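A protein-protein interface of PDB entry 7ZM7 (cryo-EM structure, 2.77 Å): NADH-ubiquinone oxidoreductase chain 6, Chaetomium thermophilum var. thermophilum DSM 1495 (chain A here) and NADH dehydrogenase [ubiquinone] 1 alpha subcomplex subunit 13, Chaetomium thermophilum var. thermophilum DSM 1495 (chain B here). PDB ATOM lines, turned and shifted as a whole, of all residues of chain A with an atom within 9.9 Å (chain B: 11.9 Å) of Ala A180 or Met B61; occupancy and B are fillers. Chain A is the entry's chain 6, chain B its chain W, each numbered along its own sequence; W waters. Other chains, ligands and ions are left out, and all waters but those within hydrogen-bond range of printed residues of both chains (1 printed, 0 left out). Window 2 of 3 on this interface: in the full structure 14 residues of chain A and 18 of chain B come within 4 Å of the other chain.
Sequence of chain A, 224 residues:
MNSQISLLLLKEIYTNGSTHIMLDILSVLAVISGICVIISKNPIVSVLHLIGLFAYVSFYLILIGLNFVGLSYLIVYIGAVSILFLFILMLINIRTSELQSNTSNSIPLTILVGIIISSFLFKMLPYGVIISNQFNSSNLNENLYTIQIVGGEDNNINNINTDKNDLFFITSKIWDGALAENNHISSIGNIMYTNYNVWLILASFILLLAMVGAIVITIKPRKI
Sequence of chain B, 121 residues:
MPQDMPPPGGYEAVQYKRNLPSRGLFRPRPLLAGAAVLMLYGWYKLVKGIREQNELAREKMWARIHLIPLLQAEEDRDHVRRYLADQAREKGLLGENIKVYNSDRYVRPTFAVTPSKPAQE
The backbone NH (N) of Trp A175 sits at hydrogen-bond distance from the side-chain amide oxygen (OE1) of Gln B72, at 3.3 Å.
The guanidinium group of Arg B64 sits at hydrogen-bond distance from the backbone carbonyl oxygen of Leu A179, at 2.5 Å.
The side-chain carboxylate (OD1) of Asp A176 lies close to the side-chain amide oxygen (OE1) of Gln B72, 3.4 Å away.
The side-chain amide oxygen (OD1) of Asn A182 lies close to the backbone carbonyl oxygen (O) of Ala A180.
Trp A175 touches Ile B68 (O to CG1, 3.8 Å).
Trp A175 touches Leu B71 (CD1 to O, 3.4 Å).
CG2 of Ile B68 touches CB of Asp A176 (3.99 Å).
Met B61 touches Leu A179 (CE to O, 3.8 Å).
Ile B68 touches Leu A179 (CD1 to CD1, 3.8 Å).
Ala A180 touches Met B61.
Of chain B, only Met B61 comes within 4 Å of Ala A180.
Met B61 touches just these residues of chain A: Leu A179 and Ala A180.
Gly A177 touches none of the printed residues of chain B.
No residue of chain B comes within 4 Å of Ala A178.
Of the printed residues of chain B, Leu A179 touches Met B61 (3.8 Å), Arg B64 (2.5 Å) and Ile B68 (3.8 Å).
No residue of chain B comes within 4 Å of Glu A181.
No residue of chain A comes within 4 Å of Ala B63.
Of the printed residues of chain B, Trp A175 touches Ile B68, Leu B71 and Gln B72.
Printed residues of chain A within 4 Å of Gln B72: Trp A175 and Asp A176.
Lys B60 touches none of the printed residues of chain A.
Gln B53 touches none of the printed residues of chain A.
The nearest residue of chain B that does not touch Ala A180 is Arg B64 (4.6 Å).
The nearest printed residue of chain A that does not touch Met B61 is Glu A181 (7.0 Å).
Of the 13 printed residues of chain A, 4 touch a printed residue of chain B.
Hydrophobic or aromatic side chains of chain A within 4 Å of the printed part of chain B: Trp A175, Leu A179 and Ala A180.
Along chain A the printed residues that touch a printed residue of chain B span positions 175 to 180.
Hydrophobic or aromatic side chains of chain B that line the printed part of chain A: Met B61, Ile B68 and Leu B71.
Among the printed residues, 9 pairs touch across the chains.
Water W1 bridges NE2 of Gln B72 and OD2 of Asp A176.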
ATOM      1  N   ILE A 174     -15.822 -34.236  20.232  1.00  0.00           N
ATOM      2  CA  ILE A 174     -14.518 -34.784  19.745  1.00  0.00           C
ATOM      3  C   ILE A 174     -14.017 -33.764  18.723  1.00  0.00           C
ATOM      4  O   ILE A 174     -14.854 -33.048  18.170  1.00  0.00           O
ATOM      5  CB  ILE A 174     -14.701 -36.179  19.110  1.00  0.00           C
ATOM      6  CG1 ILE A 174     -13.387 -36.948  18.970  1.00  0.00           C
ATOM      7  CG2 ILE A 174     -15.444 -36.095  17.785  1.00  0.00           C
ATOM      8  CD1 ILE A 174     -13.523 -38.217  18.168  1.00  0.00           C
ATOM      9  N   TRP A 175     -12.707 -33.657  18.522  1.00  0.00           N
ATOM     10  CA  TRP A 175     -12.185 -32.607  17.617  1.00  0.00           C
ATOM     11  C   TRP A 175     -11.504 -33.224  16.399  1.00  0.00           C
ATOM     12  O   TRP A 175     -11.754 -32.754  15.285  1.00  0.00           O
ATOM     13  CB  TRP A 175     -11.273 -31.666  18.398  1.00  0.00           C
ATOM     14  CG  TRP A 175     -12.008 -30.887  19.444  1.00  0.00           C
ATOM     15  CD1 TRP A 175     -12.060 -31.145  20.782  1.00  0.00           C
ATOM     16  CD2 TRP A 175     -12.833 -29.728  19.230  1.00  0.00           C
ATOM     17  NE1 TRP A 175     -12.838 -30.218  21.416  1.00  0.00           N
ATOM     18  CE2 TRP A 175     -13.329 -29.337  20.490  1.00  0.00           C
ATOM     19  CE3 TRP A 175     -13.192 -28.983  18.102  1.00  0.00           C
ATOM     20  CZ2 TRP A 175     -14.161 -28.233  20.651  1.00  0.00           C
ATOM     21  CZ3 TRP A 175     -14.012 -27.891  18.262  1.00  0.00           C
ATOM     22  CH2 TRP A 175     -14.485 -27.521  19.519  1.00  0.00           C
ATOM     23  N   ASP A 176     -10.702 -34.259  16.605  1.00  0.00           N
ATOM     24  CA  ASP A 176     -10.027 -34.969  15.486  1.00  0.00           C
ATOM     25  C   ASP A 176     -11.074 -35.600  14.563  1.00  0.00           C
ATOM     26  O   ASP A 176     -10.844 -35.596  13.341  1.00  0.00           O
ATOM     27  CB  ASP A 176      -8.933 -35.923  15.979  1.00  0.00           C
ATOM     28  CG  ASP A 176      -9.275 -36.747  17.209  1.00  0.00           C
ATOM     29  OD1 ASP A 176     -10.472 -36.923  17.490  1.00  0.00           O
ATOM     30  OD2 ASP A 176      -8.330 -37.218  17.871  1.00  0.00           O
ATOM     31  N   GLY A 177     -12.170 -36.114  15.122  1.00  0.00           N
ATOM     32  CA  GLY A 177     -13.244 -36.747  14.335  1.00  0.00           C
ATOM     33  C   GLY A 177     -14.275 -35.764  13.808  1.00  0.00           C
ATOM     34  O   GLY A 177     -15.196 -36.210  13.116  1.00  0.00           O
ATOM     35  N   ALA A 178     -14.140 -34.475  14.127  1.00  0.00           N
ATOM     36  CA  ALA A 178     -15.095 -33.439  13.668  1.00  0.00           C
ATOM     37  C   ALA A 178     -14.436 -32.484  12.672  1.00  0.00           C
ATOM     38  O   ALA A 178     -15.000 -31.419  12.455  1.00  0.00           O
ATOM     39  CB  ALA A 178     -15.632 -32.684  14.856  1.00  0.00           C
ATOM     40  N   LEU A 179     -13.297 -32.849  12.086  1.00  0.00           N
ATOM     41  CA  LEU A 179     -12.545 -31.946  11.163  1.00  0.00           C
ATOM     42  C   LEU A 179     -13.391 -31.622   9.929  1.00  0.00           C
ATOM     43  O   LEU A 179     -13.644 -30.437   9.686  1.00  0.00           O
ATOM     44  CB  LEU A 179     -11.223 -32.591  10.747  1.00  0.00           C
ATOM     45  CG  LEU A 179     -10.462 -31.884   9.624  1.00  0.00           C
ATOM     46  CD1 LEU A 179      -9.868 -30.571  10.101  1.00  0.00           C
ATOM     47  CD2 LEU A 179      -9.373 -32.774   9.053  1.00  0.00           C
ATOM     48  N   ALA A 180     -13.831 -32.650   9.208  1.00  0.00           N
ATOM     49  CA  ALA A 180     -14.670 -32.443   8.014  1.00  0.00           C
ATOM     50  C   ALA A 180     -15.854 -33.406   8.070  1.00  0.00           C
ATOM     51  O   ALA A 180     -15.888 -34.344   7.279  1.00  0.00           O
ATOM     52  CB  ALA A 180     -13.838 -32.631   6.779  1.00  0.00           C
ATOM     53  N   GLU A 181     -16.805 -33.164   8.962  1.00  0.00           N
ATOM     54  CA  GLU A 181     -17.962 -34.074   9.142  1.00  0.00           C
ATOM     55  C   GLU A 181     -18.824 -34.114   7.882  1.00  0.00           C
ATOM     56  O   GLU A 181     -18.967 -33.076   7.208  1.00  0.00           O
ATOM     57  CB  GLU A 181     -18.775 -33.691  10.376  1.00  0.00           C
ATOM     58  CG  GLU A 181     -20.000 -34.545  10.629  1.00  0.00           C
ATOM     59  CD  GLU A 181     -21.328 -33.823  10.476  1.00  0.00           C
ATOM     60  OE1 GLU A 181     -22.352 -34.380  10.918  1.00  0.00           O
ATOM     61  OE2 GLU A 181     -21.337 -32.709   9.913  1.00  0.00           O
ATOM     62  N   ASN A 182     -19.388 -35.280   7.590  1.00  0.00           N
ATOM     63  CA  ASN A 182     -20.185 -35.441   6.360  1.00  0.00           C
ATOM     64  C   ASN A 182     -21.623 -35.725   6.761  1.00  0.00           C
ATOM     65  O   ASN A 182     -21.825 -36.342   7.815  1.00  0.00           O
ATOM     66  CB  ASN A 182     -19.636 -36.554   5.465  1.00  0.00           C
ATOM     67  CG  ASN A 182     -18.178 -36.388   5.107  1.00  0.00           C
ATOM     68  OD1 ASN A 182     -17.663 -35.274   5.043  1.00  0.00           O
ATOM     69  ND2 ASN A 182     -17.504 -37.497   4.863  1.00  0.00           N
ATOM     70  N   ASN A 183     -22.573 -35.252   5.960  1.00  0.00           N
ATOM     71  CA  ASN A 183     -23.990 -35.604   6.200  1.00  0.00           C
ATOM     72  C   ASN A 183     -24.138 -37.087   5.868  1.00  0.00           C
ATOM     73  O   ASN A 183     -23.285 -37.606   5.141  1.00  0.00           O
ATOM     74  CB  ASN A 183     -24.911 -34.741   5.344  1.00  0.00           C
ATOM     75  CG  ASN A 183     -24.792 -33.266   5.651  1.00  0.00           C
ATOM     76  OD1 ASN A 183     -24.766 -32.871   6.813  1.00  0.00           O
ATOM     77  ND2 ASN A 183     -24.729 -32.447   4.614  1.00  0.00           N
ATOM     78  N   SER A 186     -23.650 -38.032   2.132  1.00  0.00           N
ATOM     79  CA  SER A 186     -22.253 -37.990   1.653  1.00  0.00           C
ATOM     80  C   SER A 186     -21.482 -39.198   2.162  1.00  0.00           C
ATOM     81  O   SER A 186     -20.679 -39.723   1.400  1.00  0.00           O
ATOM     82  CB  SER A 186     -21.634 -36.703   2.050  1.00  0.00           C
ATOM     83  OG  SER A 186     -22.347 -35.616   1.481  1.00  0.00           O
ATOM     84  N   SER A 187     -21.723 -39.605   3.403  1.00  0.00           N
ATOM     85  CA  SER A 187     -21.098 -40.834   3.941  1.00  0.00           C
ATOM     86  C   SER A 187     -21.574 -42.074   3.163  1.00  0.00           C
ATOM     87  O   SER A 187     -20.725 -42.918   2.873  1.00  0.00           O
ATOM     88  CB  SER A 187     -21.355 -40.917   5.405  1.00  0.00           C
ATOM     89  OG  SER A 187     -21.191 -39.647   6.006  1.00  0.00           O
ATOM     90  N   ASN A 190     -19.802 -41.898  -0.241  1.00  0.00           N
ATOM     91  CA  ASN A 190     -18.344 -42.171  -0.196  1.00  0.00           C
ATOM     92  C   ASN A 190     -18.118 -43.668  -0.402  1.00  0.00           C
ATOM     93  O   ASN A 190     -17.045 -44.027  -0.878  1.00  0.00           O
ATOM     94  CB  ASN A 190     -17.697 -41.721   1.116  1.00  0.00           C
ATOM     95  CG  ASN A 190     -17.702 -40.227   1.349  1.00  0.00           C
ATOM     96  OD1 ASN A 190     -17.774 -39.439   0.410  1.00  0.00           O
ATOM     97  ND2 ASN A 190     -17.623 -39.826   2.607  1.00  0.00           N
ATOM     98  N   GLU B  52     -10.902 -22.157  -7.169  1.00  0.00           N
ATOM     99  CA  GLU B  52     -10.726 -21.258  -5.996  1.00  0.00           C
ATOM    100  C   GLU B  52     -11.465 -21.815  -4.776  1.00  0.00           C
ATOM    101  O   GLU B  52     -10.899 -21.737  -3.677  1.00  0.00           O
ATOM    102  CB  GLU B  52     -11.195 -19.843  -6.341  1.00  0.00           C
ATOM    103  CG  GLU B  52     -11.316 -18.911  -5.151  1.00  0.00           C
ATOM    104  CD  GLU B  52     -10.946 -17.463  -5.423  1.00  0.00           C
ATOM    105  OE1 GLU B  52     -10.186 -17.213  -6.383  1.00  0.00           O
ATOM    106  OE2 GLU B  52     -11.415 -16.588  -4.672  1.00  0.00           O
ATOM    107  N   GLN B  53     -12.657 -22.374  -4.963  1.00  0.00           N
ATOM    108  CA  GLN B  53     -13.425 -22.935  -3.830  1.00  0.00           C
ATOM    109  C   GLN B  53     -12.608 -24.056  -3.202  1.00  0.00           C
ATOM    110  O   GLN B  53     -12.507 -24.096  -1.978  1.00  0.00           O
ATOM    111  CB  GLN B  53     -14.720 -23.577  -4.317  1.00  0.00           C
ATOM    112  CG  GLN B  53     -15.981 -22.927  -3.783  1.00  0.00           C
ATOM    113  CD  GLN B  53     -17.193 -23.590  -4.387  1.00  0.00           C
ATOM    114  OE1 GLN B  53     -17.115 -24.695  -4.910  1.00  0.00           O
ATOM    115  NE2 GLN B  53     -18.328 -22.917  -4.314  1.00  0.00           N
ATOM    116  N   ASN B  54     -12.016 -24.909  -4.023  1.00  0.00           N
ATOM    117  CA  ASN B  54     -11.225 -26.064  -3.536  1.00  0.00           C
ATOM    118  C   ASN B  54     -10.006 -25.564  -2.759  1.00  0.00           C
ATOM    119  O   ASN B  54      -9.647 -26.204  -1.774  1.00  0.00           O
ATOM    120  CB  ASN B  54     -10.921 -27.001  -4.700  1.00  0.00           C
ATOM    121  CG  ASN B  54     -12.113 -27.827  -5.126  1.00  0.00           C
ATOM    122  OD1 ASN B  54     -13.049 -28.013  -4.359  1.00  0.00           O
ATOM    123  ND2 ASN B  54     -12.086 -28.341  -6.344  1.00  0.00           N
ATOM    124  N   GLU B  55      -9.377 -24.491  -3.223  1.00  0.00           N
ATOM    125  CA  GLU B  55      -8.217 -23.878  -2.529  1.00  0.00           C
ATOM    126  C   GLU B  55      -8.638 -23.226  -1.204  1.00  0.00           C
ATOM    127  O   GLU B  55      -7.848 -23.265  -0.247  1.00  0.00           O
ATOM    128  CB  GLU B  55      -7.433 -23.018  -3.522  1.00  0.00           C
ATOM    129  CG  GLU B  55      -6.750 -23.836  -4.598  1.00  0.00           C
ATOM    130  CD  GLU B  55      -6.177 -25.153  -4.104  1.00  0.00           C
ATOM    131  OE1 GLU B  55      -5.434 -25.139  -3.100  1.00  0.00           O
ATOM    132  OE2 GLU B  55      -6.478 -26.193  -4.721  1.00  0.00           O
ATOM    133  N   LEU B  56      -9.820 -22.616  -1.155  1.00  0.00           N
ATOM    134  CA  LEU B  56     -10.340 -22.061   0.122  1.00  0.00           C
ATOM    135  C   LEU B  56     -10.561 -23.207   1.103  1.00  0.00           C
ATOM    136  O   LEU B  56     -10.297 -23.022   2.293  1.00  0.00           O
ATOM    137  CB  LEU B  56     -11.622 -21.268  -0.142  1.00  0.00           C
ATOM    138  CG  LEU B  56     -11.440 -19.957  -0.898  1.00  0.00           C
ATOM    139  CD1 LEU B  56     -12.786 -19.364  -1.277  1.00  0.00           C
ATOM    140  CD2 LEU B  56     -10.625 -18.975  -0.080  1.00  0.00           C
ATOM    141  N   ALA B  57     -11.033 -24.347   0.616  1.00  0.00           N
ATOM    142  CA  ALA B  57     -11.210 -25.539   1.470  1.00  0.00           C
ATOM    143  C   ALA B  57      -9.872 -26.061   2.022  1.00  0.00           C
ATOM    144  O   ALA B  57      -9.859 -26.507   3.170  1.00  0.00           O
ATOM    145  CB  ALA B  57     -12.009 -26.592   0.753  1.00  0.00           C
ATOM    146  N   ARG B  58      -8.794 -26.017   1.243  1.00  0.00           N
ATOM    147  CA  ARG B  58      -7.471 -26.448   1.757  1.00  0.00           C
ATOM    148  C   ARG B  58      -7.061 -25.568   2.940  1.00  0.00           C
ATOM    149  O   ARG B  58      -6.556 -26.123   3.922  1.00  0.00           O
ATOM    150  CB  ARG B  58      -6.421 -26.440   0.648  1.00  0.00           C
ATOM    151  CG  ARG B  58      -5.121 -27.131   1.024  1.00  0.00           C
ATOM    152  CD  ARG B  58      -4.054 -26.967  -0.038  1.00  0.00           C
ATOM    153  NE  ARG B  58      -4.584 -27.259  -1.357  1.00  0.00           N
ATOM    154  CZ  ARG B  58      -4.611 -28.462  -1.911  1.00  0.00           C
ATOM    155  NH1 ARG B  58      -5.121 -28.616  -3.119  1.00  0.00           N
ATOM    156  NH2 ARG B  58      -4.134 -29.505  -1.258  1.00  0.00           N
ATOM    157  N   GLU B  59      -7.303 -24.260   2.849  1.00  0.00           N
ATOM    158  CA  GLU B  59      -6.972 -23.309   3.940  1.00  0.00           C
ATOM    159  C   GLU B  59      -7.869 -23.574   5.152  1.00  0.00           C
ATOM    160  O   GLU B  59      -7.336 -23.619   6.264  1.00  0.00           O
ATOM    161  CB  GLU B  59      -7.194 -21.883   3.444  1.00  0.00           C
ATOM    162  CG  GLU B  59      -6.893 -20.808   4.469  1.00  0.00           C
ATOM    163  CD  GLU B  59      -7.079 -19.401   3.933  1.00  0.00           C
ATOM    164  OE1 GLU B  59      -6.649 -18.448   4.610  1.00  0.00           O
ATOM    165  OE2 GLU B  59      -7.659 -19.263   2.840  1.00  0.00           O
ATOM    166  N   LYS B  60      -9.170 -23.748   4.933  1.00  0.00           N
ATOM    167  CA  LYS B  60     -10.099 -24.058   6.045  1.00  0.00           C
ATOM    168  C   LYS B  60      -9.631 -25.311   6.778  1.00  0.00           C
ATOM    169  O   LYS B  60      -9.625 -25.280   8.014  1.00  0.00           O
ATOM    170  CB  LYS B  60     -11.534 -24.204   5.537  1.00  0.00           C
ATOM    171  CG  LYS B  60     -12.610 -24.164   6.610  1.00  0.00           C
ATOM    172  CD  LYS B  60     -13.930 -24.744   6.166  1.00  0.00           C
ATOM    173  CE  LYS B  60     -15.118 -23.957   6.669  1.00  0.00           C
ATOM    174  NZ  LYS B  60     -15.186 -22.616   6.042  1.00  0.00           N
ATOM    175  N   MET B  61      -9.265 -26.368   6.061  1.00  0.00           N
ATOM    176  CA  MET B  61      -8.894 -27.647   6.704  1.00  0.00           C
ATOM    177  C   MET B  61      -7.579 -27.460   7.454  1.00  0.00           C
ATOM    178  O   MET B  61      -7.507 -27.866   8.605  1.00  0.00           O
ATOM    179  CB  MET B  61      -8.769 -28.793   5.695  1.00  0.00           C
ATOM    180  CG  MET B  61     -10.084 -29.234   5.086  1.00  0.00           C
ATOM    181  SD  MET B  61     -11.253 -29.933   6.279  1.00  0.00           S
ATOM    182  CE  MET B  61     -12.095 -28.455   6.840  1.00  0.00           C
ATOM    183  N   TRP B  62      -6.594 -26.826   6.821  1.00  0.00           N
ATOM    184  CA  TRP B  62      -5.317 -26.651   7.492  1.00  0.00           C
ATOM    185  C   TRP B  62      -5.435 -25.719   8.683  1.00  0.00           C
ATOM    186  O   TRP B  62      -4.676 -25.846   9.644  1.00  0.00           O
ATOM    187  CB  TRP B  62      -4.281 -26.140   6.494  1.00  0.00           C
ATOM    188  CG  TRP B  62      -3.680 -27.254   5.718  1.00  0.00           C
ATOM    189  CD1 TRP B  62      -3.893 -27.555   4.416  1.00  0.00           C
ATOM    190  CD2 TRP B  62      -2.783 -28.244   6.216  1.00  0.00           C
ATOM    191  NE1 TRP B  62      -3.178 -28.664   4.064  1.00  0.00           N
ATOM    192  CE2 TRP B  62      -2.485 -29.105   5.155  1.00  0.00           C
ATOM    193  CE3 TRP B  62      -2.193 -28.473   7.454  1.00  0.00           C
ATOM    194  CZ2 TRP B  62      -1.631 -30.173   5.296  1.00  0.00           C
ATOM    195  CZ3 TRP B  62      -1.354 -29.525   7.588  1.00  0.00           C
ATOM    196  CH2 TRP B  62      -1.078 -30.369   6.523  1.00  0.00           C
ATOM    197  N   ALA B  63      -6.424 -24.831   8.686  1.00  0.00           N
ATOM    198  CA  ALA B  63      -6.659 -23.942   9.843  1.00  0.00           C
ATOM    199  C   ALA B  63      -7.231 -24.764  11.001  1.00  0.00           C
ATOM    200  O   ALA B  63      -6.768 -24.576  12.137  1.00  0.00           O
ATOM    201  CB  ALA B  63      -7.588 -22.843   9.428  1.00  0.00           C
ATOM    202  N   ARG B  64      -8.093 -25.761  10.764  1.00  0.00           N
ATOM    203  CA  ARG B  64      -8.651 -26.639  11.828  1.00  0.00           C
ATOM    204  C   ARG B  64      -7.643 -27.699  12.296  1.00  0.00           C
ATOM    205  O   ARG B  64      -7.715 -28.053  13.465  1.00  0.00           O
ATOM    206  CB  ARG B  64      -9.993 -27.252  11.419  1.00  0.00           C
ATOM    207  CG  ARG B  64     -11.116 -26.271  11.147  1.00  0.00           C
ATOM    208  CD  ARG B  64     -12.266 -27.145  10.709  1.00  0.00           C
ATOM    209  NE  ARG B  64     -13.467 -26.367  10.495  1.00  0.00           N
ATOM    210  CZ  ARG B  64     -14.630 -26.876  10.152  1.00  0.00           C
ATOM    211  NH1 ARG B  64     -15.675 -26.088   9.998  1.00  0.00           N
ATOM    212  NH2 ARG B  64     -14.755 -28.175   9.982  1.00  0.00           N
ATOM    213  N   ILE B  65      -6.783 -28.220  11.415  1.00  0.00           N
ATOM    214  CA  ILE B  65      -5.593 -29.013  11.844  1.00  0.00           C
ATOM    215  C   ILE B  65      -4.672 -28.364  12.874  1.00  0.00           C
ATOM    216  O   ILE B  65      -4.370 -29.034  13.863  1.00  0.00           O
ATOM    217  CB  ILE B  65      -4.842 -29.541  10.607  1.00  0.00           C
ATOM    218  CG1 ILE B  65      -5.669 -30.591   9.864  1.00  0.00           C
ATOM    219  CG2 ILE B  65      -3.453 -30.046  10.972  1.00  0.00           C
ATOM    220  CD1 ILE B  65      -5.386 -30.665   8.384  1.00  0.00           C
ATOM    221  N   HIS B  66      -4.267 -27.107  12.708  1.00  0.00           N
ATOM    222  CA  HIS B  66      -3.298 -26.530  13.678  1.00  0.00           C
ATOM    223  C   HIS B  66      -3.962 -26.355  15.049  1.00  0.00           C
ATOM    224  O   HIS B  66      -3.223 -26.188  16.029  1.00  0.00           O
ATOM    225  CB  HIS B  66      -2.665 -25.247  13.136  1.00  0.00           C
ATOM    226  CG  HIS B  66      -1.972 -25.413  11.827  1.00  0.00           C
ATOM    227  ND1 HIS B  66      -1.201 -26.519  11.533  1.00  0.00           N
ATOM    228  CD2 HIS B  66      -1.910 -24.609  10.744  1.00  0.00           C
ATOM    229  CE1 HIS B  66      -0.705 -26.397  10.320  1.00  0.00           C
ATOM    230  NE2 HIS B  66      -1.126 -25.234   9.814  1.00  0.00           N
ATOM    231  N   LEU B  67      -5.296 -26.387  15.115  1.00  0.00           N
ATOM    232  CA  LEU B  67      -6.033 -26.304  16.396  1.00  0.00           C
ATOM    233  C   LEU B  67      -6.474 -27.666  16.929  1.00  0.00           C
ATOM    234  O   LEU B  67      -6.777 -27.724  18.107  1.00  0.00           O
ATOM    235  CB  LEU B  67      -7.262 -25.447  16.132  1.00  0.00           C
ATOM    236  CG  LEU B  67      -7.006 -24.031  15.645  1.00  0.00           C
ATOM    237  CD1 LEU B  67      -8.307 -23.433  15.146  1.00  0.00           C
ATOM    238  CD2 LEU B  67      -6.389 -23.188  16.747  1.00  0.00           C
ATOM    239  N   ILE B  68      -6.494 -28.723  16.120  1.00  0.00           N
ATOM    240  CA  ILE B  68      -7.065 -30.032  16.571  1.00  0.00           C
ATOM    241  C   ILE B  68      -6.304 -30.583  17.783  1.00  0.00           C
ATOM    242  O   ILE B  68      -6.986 -31.020  18.706  1.00  0.00           O
ATOM    243  CB  ILE B  68      -7.181 -31.051  15.417  1.00  0.00           C
ATOM    244  CG1 ILE B  68      -8.518 -30.952  14.685  1.00  0.00           C
ATOM    245  CG2 ILE B  68      -6.928 -32.475  15.889  1.00  0.00           C
ATOM    246  CD1 ILE B  68      -8.580 -31.782  13.430  1.00  0.00           C
ATOM    247  N   PRO B  69      -4.950 -30.573  17.858  1.00  0.00           N
ATOM    248  CA  PRO B  69      -4.245 -31.046  19.053  1.00  0.00           C
ATOM    249  C   PRO B  69      -4.486 -30.268  20.358  1.00  0.00           C
ATOM    250  O   PRO B  69      -4.639 -30.926  21.323  1.00  0.00           O
ATOM    251  CB  PRO B  69      -2.777 -31.133  18.597  1.00  0.00           C
ATOM    252  CG  PRO B  69      -2.860 -31.178  17.100  1.00  0.00           C
ATOM    253  CD  PRO B  69      -4.000 -30.242  16.792  1.00  0.00           C
ATOM    254  N   LEU B  71      -7.269 -28.520  21.103  1.00  0.00           N
ATOM    255  CA  LEU B  71      -8.675 -28.761  21.504  1.00  0.00           C
ATOM    256  C   LEU B  71      -8.837 -30.182  22.031  1.00  0.00           C
ATOM    257  O   LEU B  71      -9.608 -30.356  22.980  1.00  0.00           O
ATOM    258  CB  LEU B  71      -9.618 -28.437  20.341  1.00  0.00           C
ATOM    259  CG  LEU B  71      -9.750 -26.957  19.997  1.00  0.00           C
ATOM    260  CD1 LEU B  71     -10.214 -26.779  18.565  1.00  0.00           C
ATOM    261  CD2 LEU B  71     -10.691 -26.264  20.962  1.00  0.00           C
ATOM    262  N   GLN B  72      -8.181 -31.153  21.402  1.00  0.00           N
ATOM    263  CA  GLN B  72      -8.239 -32.572  21.810  1.00  0.00           C
ATOM    264  C   GLN B  72      -7.575 -32.753  23.169  1.00  0.00           C
ATOM    265  O   GLN B  72      -8.091 -33.529  23.966  1.00  0.00           O
ATOM    266  CB  GLN B  72      -7.599 -33.420  20.712  1.00  0.00           C
ATOM    267  CG  GLN B  72      -7.804 -34.915  20.891  1.00  0.00           C
ATOM    268  CD  GLN B  72      -9.263 -35.290  20.839  1.00  0.00           C
ATOM    269  OE1 GLN B  72     -10.045 -34.743  20.066  1.00  0.00           O
ATOM    270  NE2 GLN B  72      -9.641 -36.247  21.667  1.00  0.00           N
HETATM  271  O   HOH W   1      -9.421 -39.077  20.519  1.00  0.00           O
